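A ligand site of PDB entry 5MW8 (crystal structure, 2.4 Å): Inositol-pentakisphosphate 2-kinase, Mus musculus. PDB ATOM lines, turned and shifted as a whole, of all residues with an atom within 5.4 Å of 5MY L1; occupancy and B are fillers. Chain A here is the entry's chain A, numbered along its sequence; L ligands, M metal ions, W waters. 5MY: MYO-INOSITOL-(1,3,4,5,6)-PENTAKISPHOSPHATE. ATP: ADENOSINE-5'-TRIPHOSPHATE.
His 167 touches 5MY L1.
CE of Met 399 touches O44 of 5MY L1 (3.7 Å).
Leu 455 touches 5MY L1.
Hydrophobic or aromatic side chains that line 5MY L1: His 167, Met 399 and Leu 455.
The nearest printed residue that does not touch 5MY L1 is Gly 20 (4.6 Å).
The guanidinium group (NE) of Arg 103 lies within hydrogen-bond range of the backbone carbonyl oxygen (O) of Gly 20, at 3.5 Å.
The side-chain amino group of Lys 141 lies within salt-bridge range of the side-chain carboxylate of Asp 403.
The side-chain carboxylate (OD2) of Asp 403 is in salt-bridge range of the side-chain amino group (NZ) of Lys 444 (3.3 Å).
OD1 of Asp 403 is in salt-bridge range of NZ of Lys 143.
The backbone carbonyl oxygen (O) of Asn 210 lies within hydrogen-bond range of the backbone NH (N) of Lys 141 (3.1 Å).
OD1 of Asn 209 sits at hydrogen-bond distance from ND2 of Asn 210, 3.3 Å away.
The backbone carbonyl oxygen of Lys 171 lies within hydrogen-bond range of the backbone NH of Lys 176 (2.9 Å).
Water W5 lies within hydrogen-bond range of NE of Arg 163, O45 of 5MY L1 and ND1 of His 167.
Water W1 lies within hydrogen-bond range of an oxygen (O21) of 5MY L1, an oxygen (O2G) of ATP L2, the side-chain amino group (NZ) of Lys 141 and the side-chain amide nitrogen (ND2) of Asn 209.
Water W2 lies within hydrogen-bond range of the side-chain amide nitrogen of Asn 210, an oxygen (O26) of 5MY L1 and the side-chain amide oxygen of Asn 209.
Water W3 lies within hydrogen-bond range of NZ of Lys 171 and O36 of 5MY L1.
NE2 of Gln 452 is in hydrogen-bond range of O34 of 5MY L1 (2.6 Å).
NH1 of Arg 103 lies within salt-bridge range of O31 of 5MY L1, 2.7 Å away.
OD2 of Asp 403 lies within hydrogen-bond range of O12 of 5MY L1, 2.7 Å away.
The side-chain amino group (NZ) of Lys 141 is in salt-bridge range of an oxygen (O26) of 5MY L1 (3.0 Å).
The side-chain amide nitrogen of Asn 209 is in hydrogen-bond range of an oxygen (O21) of 5MY L1 (2.7 Å).
OD1 of Asn 21 lies close to O23 of 5MY L1 (2.8 Å).
NZ of Lys 171 lies within salt-bridge range of O36 of 5MY L1 (2.8 Å).
An oxygen (O43) of 5MY L1 lies within salt-bridge range of the side-chain amino group (NZ) of Lys 444 (3.1 Å).
NZ of Lys 143 lies within salt-bridge range of O26 of 5MY L1, at 3.4 Å.
NZ of Lys 22 is in salt-bridge range of O33 of 5MY L1, at 3.7 Å.
An oxygen (O41) of 5MY L1 is in salt-bridge range of the side-chain amino group (NZ) of Lys 176 (3.4 Å).
The guanidinium group (NH2) of Arg 163 is in salt-bridge range of an oxygen (O35) of 5MY L1 (3.6 Å).
The side-chain amino group (NZ) of Lys 141 sits close to an oxygen (O3G) of ATP L2 (3.5 Å).
The backbone NH (N) of Lys 22 is in hydrogen-bond range of an oxygen (O2B) of ATP L2, 3.2 Å away.
The backbone NH (N) of Gly 20 sits close to an oxygen (O2B) of ATP L2 (3.4 Å).
An oxygen (O12) of 5MY L1 is in hydrogen-bond range of an oxygen (O2G) of ATP L2 (3.1 Å).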
ATOM      1  N   GLY A  20     -27.194 -29.592 -35.076  1.00  0.00           N
ATOM      2  CA  GLY A  20     -26.359 -28.536 -34.497  1.00  0.00           C
ATOM      3  C   GLY A  20     -24.946 -29.059 -34.504  1.00  0.00           C
ATOM      4  O   GLY A  20     -24.578 -29.798 -35.420  1.00  0.00           O
ATOM      5  N   ASN A  21     -24.150 -28.715 -33.484  1.00  0.00           N
ATOM      6  CA  ASN A  21     -22.797 -29.311 -33.346  1.00  0.00           C
ATOM      7  C   ASN A  21     -22.657 -30.348 -32.228  1.00  0.00           C
ATOM      8  O   ASN A  21     -21.567 -30.875 -32.032  1.00  0.00           O
ATOM      9  CB  ASN A  21     -21.683 -28.257 -33.244  1.00  0.00           C
ATOM     10  CG  ASN A  21     -21.801 -27.390 -32.020  1.00  0.00           C
ATOM     11  OD1 ASN A  21     -22.719 -26.598 -31.919  1.00  0.00           O
ATOM     12  ND2 ASN A  21     -20.859 -27.524 -31.101  1.00  0.00           N
ATOM     13  N   LYS A  22     -23.738 -30.641 -31.498  1.00  0.00           N
ATOM     14  CA  LYS A  22     -23.752 -31.771 -30.560  1.00  0.00           C
ATOM     15  C   LYS A  22     -24.440 -33.009 -31.114  1.00  0.00           C
ATOM     16  O   LYS A  22     -24.005 -34.127 -30.837  1.00  0.00           O
ATOM     17  CB  LYS A  22     -24.418 -31.390 -29.234  1.00  0.00           C
ATOM     18  CG  LYS A  22     -23.686 -30.340 -28.416  1.00  0.00           C
ATOM     19  CD  LYS A  22     -22.224 -30.665 -28.189  1.00  0.00           C
ATOM     20  CE  LYS A  22     -21.637 -29.877 -27.021  1.00  0.00           C
ATOM     21  NZ  LYS A  22     -20.245 -29.418 -27.311  1.00  0.00           N
ATOM     22  N   ARG A 103     -20.380 -28.538 -40.870  1.00  0.00           N
ATOM     23  CA  ARG A 103     -20.626 -29.468 -39.762  1.00  0.00           C
ATOM     24  C   ARG A 103     -19.808 -30.763 -39.831  1.00  0.00           C
ATOM     25  O   ARG A 103     -19.694 -31.465 -38.828  1.00  0.00           O
ATOM     26  CB  ARG A 103     -22.111 -29.859 -39.700  1.00  0.00           C
ATOM     27  CG  ARG A 103     -23.077 -28.701 -39.448  1.00  0.00           C
ATOM     28  CD  ARG A 103     -22.887 -28.065 -38.088  1.00  0.00           C
ATOM     29  NE  ARG A 103     -24.029 -27.234 -37.710  1.00  0.00           N
ATOM     30  CZ  ARG A 103     -24.062 -26.403 -36.664  1.00  0.00           C
ATOM     31  NH1 ARG A 103     -23.016 -26.256 -35.862  1.00  0.00           N
ATOM     32  NH2 ARG A 103     -25.173 -25.707 -36.432  1.00  0.00           N
ATOM     33  N   LYS A 141     -34.712 -20.130 -32.822  1.00  0.00           N
ATOM     34  CA  LYS A 141     -33.701 -20.172 -31.771  1.00  0.00           C
ATOM     35  C   LYS A 141     -33.595 -18.726 -31.268  1.00  0.00           C
ATOM     36  O   LYS A 141     -32.825 -17.930 -31.817  1.00  0.00           O
ATOM     37  CB  LYS A 141     -32.380 -20.672 -32.351  1.00  0.00           C
ATOM     38  CG  LYS A 141     -31.485 -21.377 -31.342  1.00  0.00           C
ATOM     39  CD  LYS A 141     -30.056 -21.480 -31.833  1.00  0.00           C
ATOM     40  CE  LYS A 141     -29.298 -22.563 -31.096  1.00  0.00           C
ATOM     41  NZ  LYS A 141     -27.824 -22.433 -31.257  1.00  0.00           N
ATOM     42  N   LYS A 143     -32.507 -17.135 -28.541  1.00  0.00           N
ATOM     43  CA  LYS A 143     -31.367 -16.683 -27.752  1.00  0.00           C
ATOM     44  C   LYS A 143     -31.791 -15.883 -26.504  1.00  0.00           C
ATOM     45  O   LYS A 143     -32.977 -15.839 -26.182  1.00  0.00           O
ATOM     46  CB  LYS A 143     -30.321 -15.971 -28.636  1.00  0.00           C
ATOM     47  CG  LYS A 143     -29.618 -16.920 -29.607  1.00  0.00           C
ATOM     48  CD  LYS A 143     -29.008 -18.099 -28.860  1.00  0.00           C
ATOM     49  CE  LYS A 143     -27.705 -18.590 -29.469  1.00  0.00           C
ATOM     50  NZ  LYS A 143     -26.940 -19.411 -28.501  1.00  0.00           N
ATOM     51  N   ARG A 163     -26.281  -9.591 -25.668  1.00  0.00           N
ATOM     52  CA  ARG A 163     -25.264 -10.556 -26.083  1.00  0.00           C
ATOM     53  C   ARG A 163     -25.349 -10.822 -27.583  1.00  0.00           C
ATOM     54  O   ARG A 163     -24.361 -10.685 -28.298  1.00  0.00           O
ATOM     55  CB  ARG A 163     -25.453 -11.856 -25.272  1.00  0.00           C
ATOM     56  CG  ARG A 163     -24.726 -13.085 -25.787  1.00  0.00           C
ATOM     57  CD  ARG A 163     -23.221 -12.894 -25.903  1.00  0.00           C
ATOM     58  NE  ARG A 163     -22.592 -14.211 -25.921  1.00  0.00           N
ATOM     59  CZ  ARG A 163     -22.132 -14.878 -24.856  1.00  0.00           C
ATOM     60  NH1 ARG A 163     -22.150 -14.347 -23.631  1.00  0.00           N
ATOM     61  NH2 ARG A 163     -21.615 -16.092 -25.032  1.00  0.00           N
ATOM     62  N   HIS A 167     -22.566 -10.064 -30.281  1.00  0.00           N
ATOM     63  CA  HIS A 167     -21.956 -11.267 -30.873  1.00  0.00           C
ATOM     64  C   HIS A 167     -21.970 -11.238 -32.406  1.00  0.00           C
ATOM     65  O   HIS A 167     -20.998 -11.637 -33.050  1.00  0.00           O
ATOM     66  CB  HIS A 167     -22.666 -12.526 -30.371  1.00  0.00           C
ATOM     67  CG  HIS A 167     -21.865 -13.789 -30.504  1.00  0.00           C
ATOM     68  ND1 HIS A 167     -22.296 -14.985 -29.974  1.00  0.00           N
ATOM     69  CD2 HIS A 167     -20.662 -14.038 -31.068  1.00  0.00           C
ATOM     70  CE1 HIS A 167     -21.395 -15.926 -30.226  1.00  0.00           C
ATOM     71  NE2 HIS A 167     -20.394 -15.370 -30.893  1.00  0.00           N
ATOM     72  N   LYS A 171     -19.144 -12.564 -35.588  1.00  0.00           N
ATOM     73  CA  LYS A 171     -19.582 -13.672 -36.449  1.00  0.00           C
ATOM     74  C   LYS A 171     -19.486 -13.305 -37.920  1.00  0.00           C
ATOM     75  O   LYS A 171     -19.091 -14.131 -38.745  1.00  0.00           O
ATOM     76  CB  LYS A 171     -21.007 -14.100 -36.092  1.00  0.00           C
ATOM     77  CG  LYS A 171     -21.151 -14.606 -34.662  1.00  0.00           C
ATOM     78  CD  LYS A 171     -22.595 -14.691 -34.186  1.00  0.00           C
ATOM     79  CE  LYS A 171     -22.991 -16.108 -33.808  1.00  0.00           C
ATOM     80  NZ  LYS A 171     -24.337 -16.156 -33.196  1.00  0.00           N
ATOM     81  N   LYS A 176     -18.830 -16.312 -40.562  1.00  0.00           N
ATOM     82  CA  LYS A 176     -19.846 -17.278 -40.162  1.00  0.00           C
ATOM     83  C   LYS A 176     -21.118 -17.003 -40.968  1.00  0.00           C
ATOM     84  O   LYS A 176     -21.738 -17.932 -41.497  1.00  0.00           O
ATOM     85  CB  LYS A 176     -20.137 -17.146 -38.669  1.00  0.00           C
ATOM     86  CG  LYS A 176     -20.988 -18.260 -38.049  1.00  0.00           C
ATOM     87  CD  LYS A 176     -20.171 -19.241 -37.216  1.00  0.00           C
ATOM     88  CE  LYS A 176     -21.010 -19.953 -36.156  1.00  0.00           C
ATOM     89  NZ  LYS A 176     -21.985 -20.918 -36.742  1.00  0.00           N
ATOM     90  N   ASN A 209     -28.851 -19.248 -38.027  1.00  0.00           N
ATOM     91  CA  ASN A 209     -29.286 -20.487 -37.371  1.00  0.00           C
ATOM     92  C   ASN A 209     -30.443 -20.241 -36.409  1.00  0.00           C
ATOM     93  O   ASN A 209     -30.732 -21.084 -35.540  1.00  0.00           O
ATOM     94  CB  ASN A 209     -28.105 -21.125 -36.616  1.00  0.00           C
ATOM     95  CG  ASN A 209     -27.633 -20.288 -35.440  1.00  0.00           C
ATOM     96  OD1 ASN A 209     -27.724 -19.051 -35.446  1.00  0.00           O
ATOM     97  ND2 ASN A 209     -27.110 -20.960 -34.408  1.00  0.00           N
ATOM     98  N   ASN A 210     -31.107 -19.108 -36.579  1.00  0.00           N
ATOM     99  CA  ASN A 210     -32.156 -18.641 -35.678  1.00  0.00           C
ATOM    100  C   ASN A 210     -33.579 -18.781 -36.228  1.00  0.00           C
ATOM    101  O   ASN A 210     -34.533 -18.552 -35.480  1.00  0.00           O
ATOM    102  CB  ASN A 210     -31.887 -17.175 -35.332  1.00  0.00           C
ATOM    103  CG  ASN A 210     -30.504 -16.952 -34.756  1.00  0.00           C
ATOM    104  OD1 ASN A 210     -29.718 -16.157 -35.277  1.00  0.00           O
ATOM    105  ND2 ASN A 210     -30.185 -17.661 -33.681  1.00  0.00           N
ATOM    106  N   MET A 399     -27.882 -21.469 -19.339  1.00  0.00           N
ATOM    107  CA  MET A 399     -27.191 -21.695 -20.618  1.00  0.00           C
ATOM    108  C   MET A 399     -28.048 -22.553 -21.563  1.00  0.00           C
ATOM    109  O   MET A 399     -28.166 -22.238 -22.752  1.00  0.00           O
ATOM    110  CB  MET A 399     -25.859 -22.427 -20.416  1.00  0.00           C
ATOM    111  CG  MET A 399     -24.687 -21.601 -19.933  1.00  0.00           C
ATOM    112  SD  MET A 399     -23.208 -22.635 -19.803  1.00  0.00           S
ATOM    113  CE  MET A 399     -22.911 -23.064 -21.511  1.00  0.00           C
ATOM    114  N   ASP A 403     -29.967 -21.405 -25.276  1.00  0.00           N
ATOM    115  CA  ASP A 403     -29.616 -22.026 -26.541  1.00  0.00           C
ATOM    116  C   ASP A 403     -30.696 -23.007 -27.051  1.00  0.00           C
ATOM    117  O   ASP A 403     -30.444 -23.802 -27.955  1.00  0.00           O
ATOM    118  CB  ASP A 403     -28.271 -22.744 -26.376  1.00  0.00           C
ATOM    119  CG  ASP A 403     -27.662 -23.183 -27.708  1.00  0.00           C
ATOM    120  OD1 ASP A 403     -27.311 -22.312 -28.526  1.00  0.00           O
ATOM    121  OD2 ASP A 403     -27.526 -24.413 -27.922  1.00  0.00           O
ATOM    122  N   ASP A 440     -34.137 -28.977 -27.893  1.00  0.00           N
ATOM    123  CA  ASP A 440     -32.722 -28.740 -27.581  1.00  0.00           C
ATOM    124  C   ASP A 440     -32.540 -28.381 -26.097  1.00  0.00           C
ATOM    125  O   ASP A 440     -32.066 -27.291 -25.755  1.00  0.00           O
ATOM    126  CB  ASP A 440     -32.160 -27.638 -28.519  1.00  0.00           C
ATOM    127  CG  ASP A 440     -30.678 -27.805 -28.810  1.00  0.00           C
ATOM    128  OD1 ASP A 440     -29.895 -28.231 -27.931  1.00  0.00           O
ATOM    129  OD2 ASP A 440     -30.295 -27.476 -29.954  1.00  0.00           O
ATOM    130  N   ASP A 442     -30.825 -30.343 -23.596  1.00  0.00           N
ATOM    131  CA  ASP A 442     -29.804 -31.124 -22.879  1.00  0.00           C
ATOM    132  C   ASP A 442     -28.946 -30.153 -22.075  1.00  0.00           C
ATOM    133  O   ASP A 442     -28.550 -29.099 -22.590  1.00  0.00           O
ATOM    134  CB  ASP A 442     -28.962 -32.056 -23.788  1.00  0.00           C
ATOM    135  CG  ASP A 442     -28.484 -31.392 -25.077  1.00  0.00           C
ATOM    136  OD1 ASP A 442     -29.254 -30.629 -25.684  1.00  0.00           O
ATOM    137  OD2 ASP A 442     -27.341 -31.692 -25.492  1.00  0.00           O
ATOM    138  N   LYS A 444     -26.209 -28.081 -20.330  1.00  0.00           N
ATOM    139  CA  LYS A 444     -24.896 -27.688 -20.804  1.00  0.00           C
ATOM    140  C   LYS A 444     -23.853 -28.170 -19.806  1.00  0.00           C
ATOM    141  O   LYS A 444     -24.126 -28.183 -18.604  1.00  0.00           O
ATOM    142  CB  LYS A 444     -24.832 -26.177 -21.001  1.00  0.00           C
ATOM    143  CG  LYS A 444     -25.700 -25.694 -22.157  1.00  0.00           C
ATOM    144  CD  LYS A 444     -24.992 -25.885 -23.482  1.00  0.00           C
ATOM    145  CE  LYS A 444     -25.714 -25.208 -24.636  1.00  0.00           C
ATOM    146  NZ  LYS A 444     -26.794 -26.043 -25.203  1.00  0.00           N
ATOM    147  N   SER A 448     -17.554 -26.450 -19.771  1.00  0.00           N
ATOM    148  CA  SER A 448     -17.569 -25.346 -20.742  1.00  0.00           C
ATOM    149  C   SER A 448     -17.632 -23.941 -20.118  1.00  0.00           C
ATOM    150  O   SER A 448     -17.602 -22.956 -20.852  1.00  0.00           O
ATOM    151  CB  SER A 448     -18.756 -25.510 -21.689  1.00  0.00           C
ATOM    152  OG  SER A 448     -19.987 -25.381 -20.992  1.00  0.00           O
ATOM    153  N   HIS A 451     -14.821 -21.560 -20.965  1.00  0.00           N
ATOM    154  CA  HIS A 451     -15.015 -21.155 -22.352  1.00  0.00           C
ATOM    155  C   HIS A 451     -15.993 -19.979 -22.474  1.00  0.00           C
ATOM    156  O   HIS A 451     -15.718 -19.021 -23.211  1.00  0.00           O
ATOM    157  CB  HIS A 451     -15.473 -22.344 -23.219  1.00  0.00           C
ATOM    158  CG  HIS A 451     -15.907 -21.953 -24.601  1.00  0.00           C
ATOM    159  ND1 HIS A 451     -15.087 -21.267 -25.460  1.00  0.00           N
ATOM    160  CD2 HIS A 451     -17.074 -22.144 -25.259  1.00  0.00           C
ATOM    161  CE1 HIS A 451     -15.727 -21.044 -26.603  1.00  0.00           C
ATOM    162  NE2 HIS A 451     -16.940 -21.570 -26.494  1.00  0.00           N
ATOM    163  N   GLN A 452     -17.095 -20.023 -21.744  1.00  0.00           N
ATOM    164  CA  GLN A 452     -18.071 -18.925 -21.717  1.00  0.00           C
ATOM    165  C   GLN A 452     -17.452 -17.621 -21.211  1.00  0.00           C
ATOM    166  O   GLN A 452     -17.768 -16.541 -21.707  1.00  0.00           O
ATOM    167  CB  GLN A 452     -19.295 -19.251 -20.859  1.00  0.00           C
ATOM    168  CG  GLN A 452     -20.119 -20.461 -21.301  1.00  0.00           C
ATOM    169  CD  GLN A 452     -20.651 -20.323 -22.712  1.00  0.00           C
ATOM    170  OE1 GLN A 452     -21.272 -19.310 -23.064  1.00  0.00           O
ATOM    171  NE2 GLN A 452     -20.421 -21.345 -23.528  1.00  0.00           N
ATOM    172  N   LEU A 455     -14.977 -16.438 -24.073  1.00  0.00           N
ATOM    173  CA  LEU A 455     -15.733 -15.984 -25.242  1.00  0.00           C
ATOM    174  C   LEU A 455     -16.405 -14.641 -24.994  1.00  0.00           C
ATOM    175  O   LEU A 455     -16.354 -13.755 -25.846  1.00  0.00           O
ATOM    176  CB  LEU A 455     -16.782 -17.038 -25.609  1.00  0.00           C
ATOM    177  CG  LEU A 455     -17.660 -16.787 -26.837  1.00  0.00           C
ATOM    178  CD1 LEU A 455     -16.807 -16.537 -28.064  1.00  0.00           C
ATOM    179  CD2 LEU A 455     -18.600 -17.968 -27.058  1.00  0.00           C
HETATM  180  O31 5MY L   1     -23.730 -24.681 -33.839  1.00  0.00           O
HETATM  181  P1  5MY L   1     -24.102 -23.216 -33.814  1.00  0.00           P
HETATM  182  O21 5MY L   1     -25.160 -22.834 -34.814  1.00  0.00           O
HETATM  183  O41 5MY L   1     -22.913 -22.290 -33.824  1.00  0.00           O
HETATM  184  O11 5MY L   1     -24.798 -22.974 -32.382  1.00  0.00           O
HETATM  185  C1  5MY L   1     -24.062 -23.035 -31.149  1.00  0.00           C
HETATM  186  C2  5MY L   1     -24.581 -24.209 -30.327  1.00  0.00           C
HETATM  187  O12 5MY L   1     -25.977 -24.057 -30.090  1.00  0.00           O
HETATM  188  C3  5MY L   1     -23.838 -24.327 -28.991  1.00  0.00           C
HETATM  189  O13 5MY L   1     -24.477 -25.306 -28.166  1.00  0.00           O
HETATM  190  P3  5MY L   1     -23.918 -26.808 -28.014  1.00  0.00           P
HETATM  191  O23 5MY L   1     -23.743 -27.245 -29.434  1.00  0.00           O
HETATM  192  O33 5MY L   1     -22.640 -26.631 -27.230  1.00  0.00           O
HETATM  193  O43 5MY L   1     -25.005 -27.558 -27.285  1.00  0.00           O
HETATM  194  C6  5MY L   1     -24.215 -21.747 -30.358  1.00  0.00           C
HETATM  195  O16 5MY L   1     -23.728 -20.662 -31.128  1.00  0.00           O
HETATM  196  P6  5MY L   1     -24.652 -19.584 -31.892  1.00  0.00           P
HETATM  197  O26 5MY L   1     -26.083 -20.020 -31.685  1.00  0.00           O
HETATM  198  O36 5MY L   1     -24.318 -18.256 -31.275  1.00  0.00           O
HETATM  199  O46 5MY L   1     -24.190 -19.681 -33.325  1.00  0.00           O
HETATM  200  C5  5MY L   1     -23.458 -21.793 -29.046  1.00  0.00           C
HETATM  201  O15 5MY L   1     -23.801 -20.647 -28.264  1.00  0.00           O
HETATM  202  P5  5MY L   1     -22.856 -19.353 -28.018  1.00  0.00           P
HETATM  203  O25 5MY L   1     -21.455 -19.720 -28.440  1.00  0.00           O
HETATM  204  O35 5MY L   1     -22.999 -19.064 -26.546  1.00  0.00           O
HETATM  205  O45 5MY L   1     -23.493 -18.308 -28.891  1.00  0.00           O
HETATM  206  C4  5MY L   1     -23.804 -23.018 -28.214  1.00  0.00           C
HETATM  207  O14 5MY L   1     -22.796 -23.150 -27.223  1.00  0.00           O
HETATM  208  P4  5MY L   1     -22.970 -22.813 -25.657  1.00  0.00           P
HETATM  209  O34 5MY L   1     -22.128 -21.588 -25.459  1.00  0.00           O
HETATM  210  O44 5MY L   1     -22.402 -24.048 -25.010  1.00  0.00           O
HETATM  211  O24 5MY L   1     -24.440 -22.566 -25.392  1.00  0.00           O
HETATM  212  PG  ATP L   2     -27.639 -26.821 -31.193  1.00  0.00           P
HETATM  213  O1G ATP L   2     -27.356 -26.969 -29.714  1.00  0.00           O
HETATM  214  O2G ATP L   2     -26.401 -26.419 -32.016  1.00  0.00           O
HETATM  215  O3G ATP L   2     -28.771 -25.843 -31.492  1.00  0.00           O
HETATM  216  PB  ATP L   2     -28.098 -29.709 -31.248  1.00  0.00           P
HETATM  217  O1B ATP L   2     -28.093 -29.678 -29.721  1.00  0.00           O
HETATM  218  O2B ATP L   2     -26.892 -30.381 -31.771  1.00  0.00           O
HETATM  219  O3B ATP L   2     -28.169 -28.208 -31.776  1.00  0.00           O
HETATM  220  PA  ATP L   2     -30.894 -30.029 -32.011  1.00  0.00           P
HETATM  221  O1A ATP L   2     -31.780 -30.352 -30.871  1.00  0.00           O
HETATM  222  O2A ATP L   2     -30.908 -28.518 -32.261  1.00  0.00           O
HETATM  223  O3A ATP L   2     -29.411 -30.489 -31.708  1.00  0.00           O
HETATM  224  O5' ATP L   2     -31.289 -30.797 -33.364  1.00  0.00           O
HETATM  225  C5' ATP L   2     -30.901 -30.386 -34.687  1.00  0.00           C
HETATM  226  C4' ATP L   2     -32.115 -29.980 -35.491  1.00  0.00           C
HETATM  227  O4' ATP L   2     -32.953 -31.130 -35.731  1.00  0.00           O
HETATM  228  C3' ATP L   2     -33.031 -28.955 -34.854  1.00  0.00           C
HETATM  229  O3' ATP L   2     -32.535 -27.639 -35.056  1.00  0.00           O
HETATM  230  C2' ATP L   2     -34.355 -29.215 -35.592  1.00  0.00           C
HETATM  231  O2' ATP L   2     -34.409 -28.589 -36.864  1.00  0.00           O
HETATM  232  C1' ATP L   2     -34.316 -30.742 -35.759  1.00  0.00           C
HETATM  233  N9  ATP L   2     -35.042 -31.478 -34.728  1.00  0.00           N
HETATM  234  C8  ATP L   2     -34.566 -31.914 -33.520  1.00  0.00           C
HETATM  235  N7  ATP L   2     -35.442 -32.589 -32.815  1.00  0.00           N
HETATM  236  C5  ATP L   2     -36.580 -32.586 -33.613  1.00  0.00           C
HETATM  237  C6  ATP L   2     -37.865 -33.132 -33.432  1.00  0.00           C
HETATM  238  N6  ATP L   2     -38.222 -33.844 -32.359  1.00  0.00           N
HETATM  239  N1  ATP L   2     -38.779 -32.921 -34.409  1.00  0.00           N
HETATM  240  C2  ATP L   2     -38.414 -32.231 -35.489  1.00  0.00           C
HETATM  241  N3  ATP L   2     -37.230 -31.685 -35.784  1.00  0.00           N
HETATM  242  C4  ATP L   2     -36.342 -31.899 -34.791  1.00  0.00           C
HETATM  243 MG    MG M   1     -27.581 -28.474 -27.722  1.00  0.00          MG
HETATM  244  O   HOH W   1     -27.263 -24.131 -33.702  1.00  0.00           O
HETATM  245  O   HOH W   2     -27.670 -17.906 -32.630  1.00  0.00           O
HETATM  246  O   HOH W   3     -26.117 -15.892 -31.250  1.00  0.00           O
HETATM  247  O   HOH W   4     -20.312 -25.108 -27.084  1.00  0.00           O
HETATM  248  O   HOH W   5     -23.727 -16.009 -27.506  1.00  0.00           O
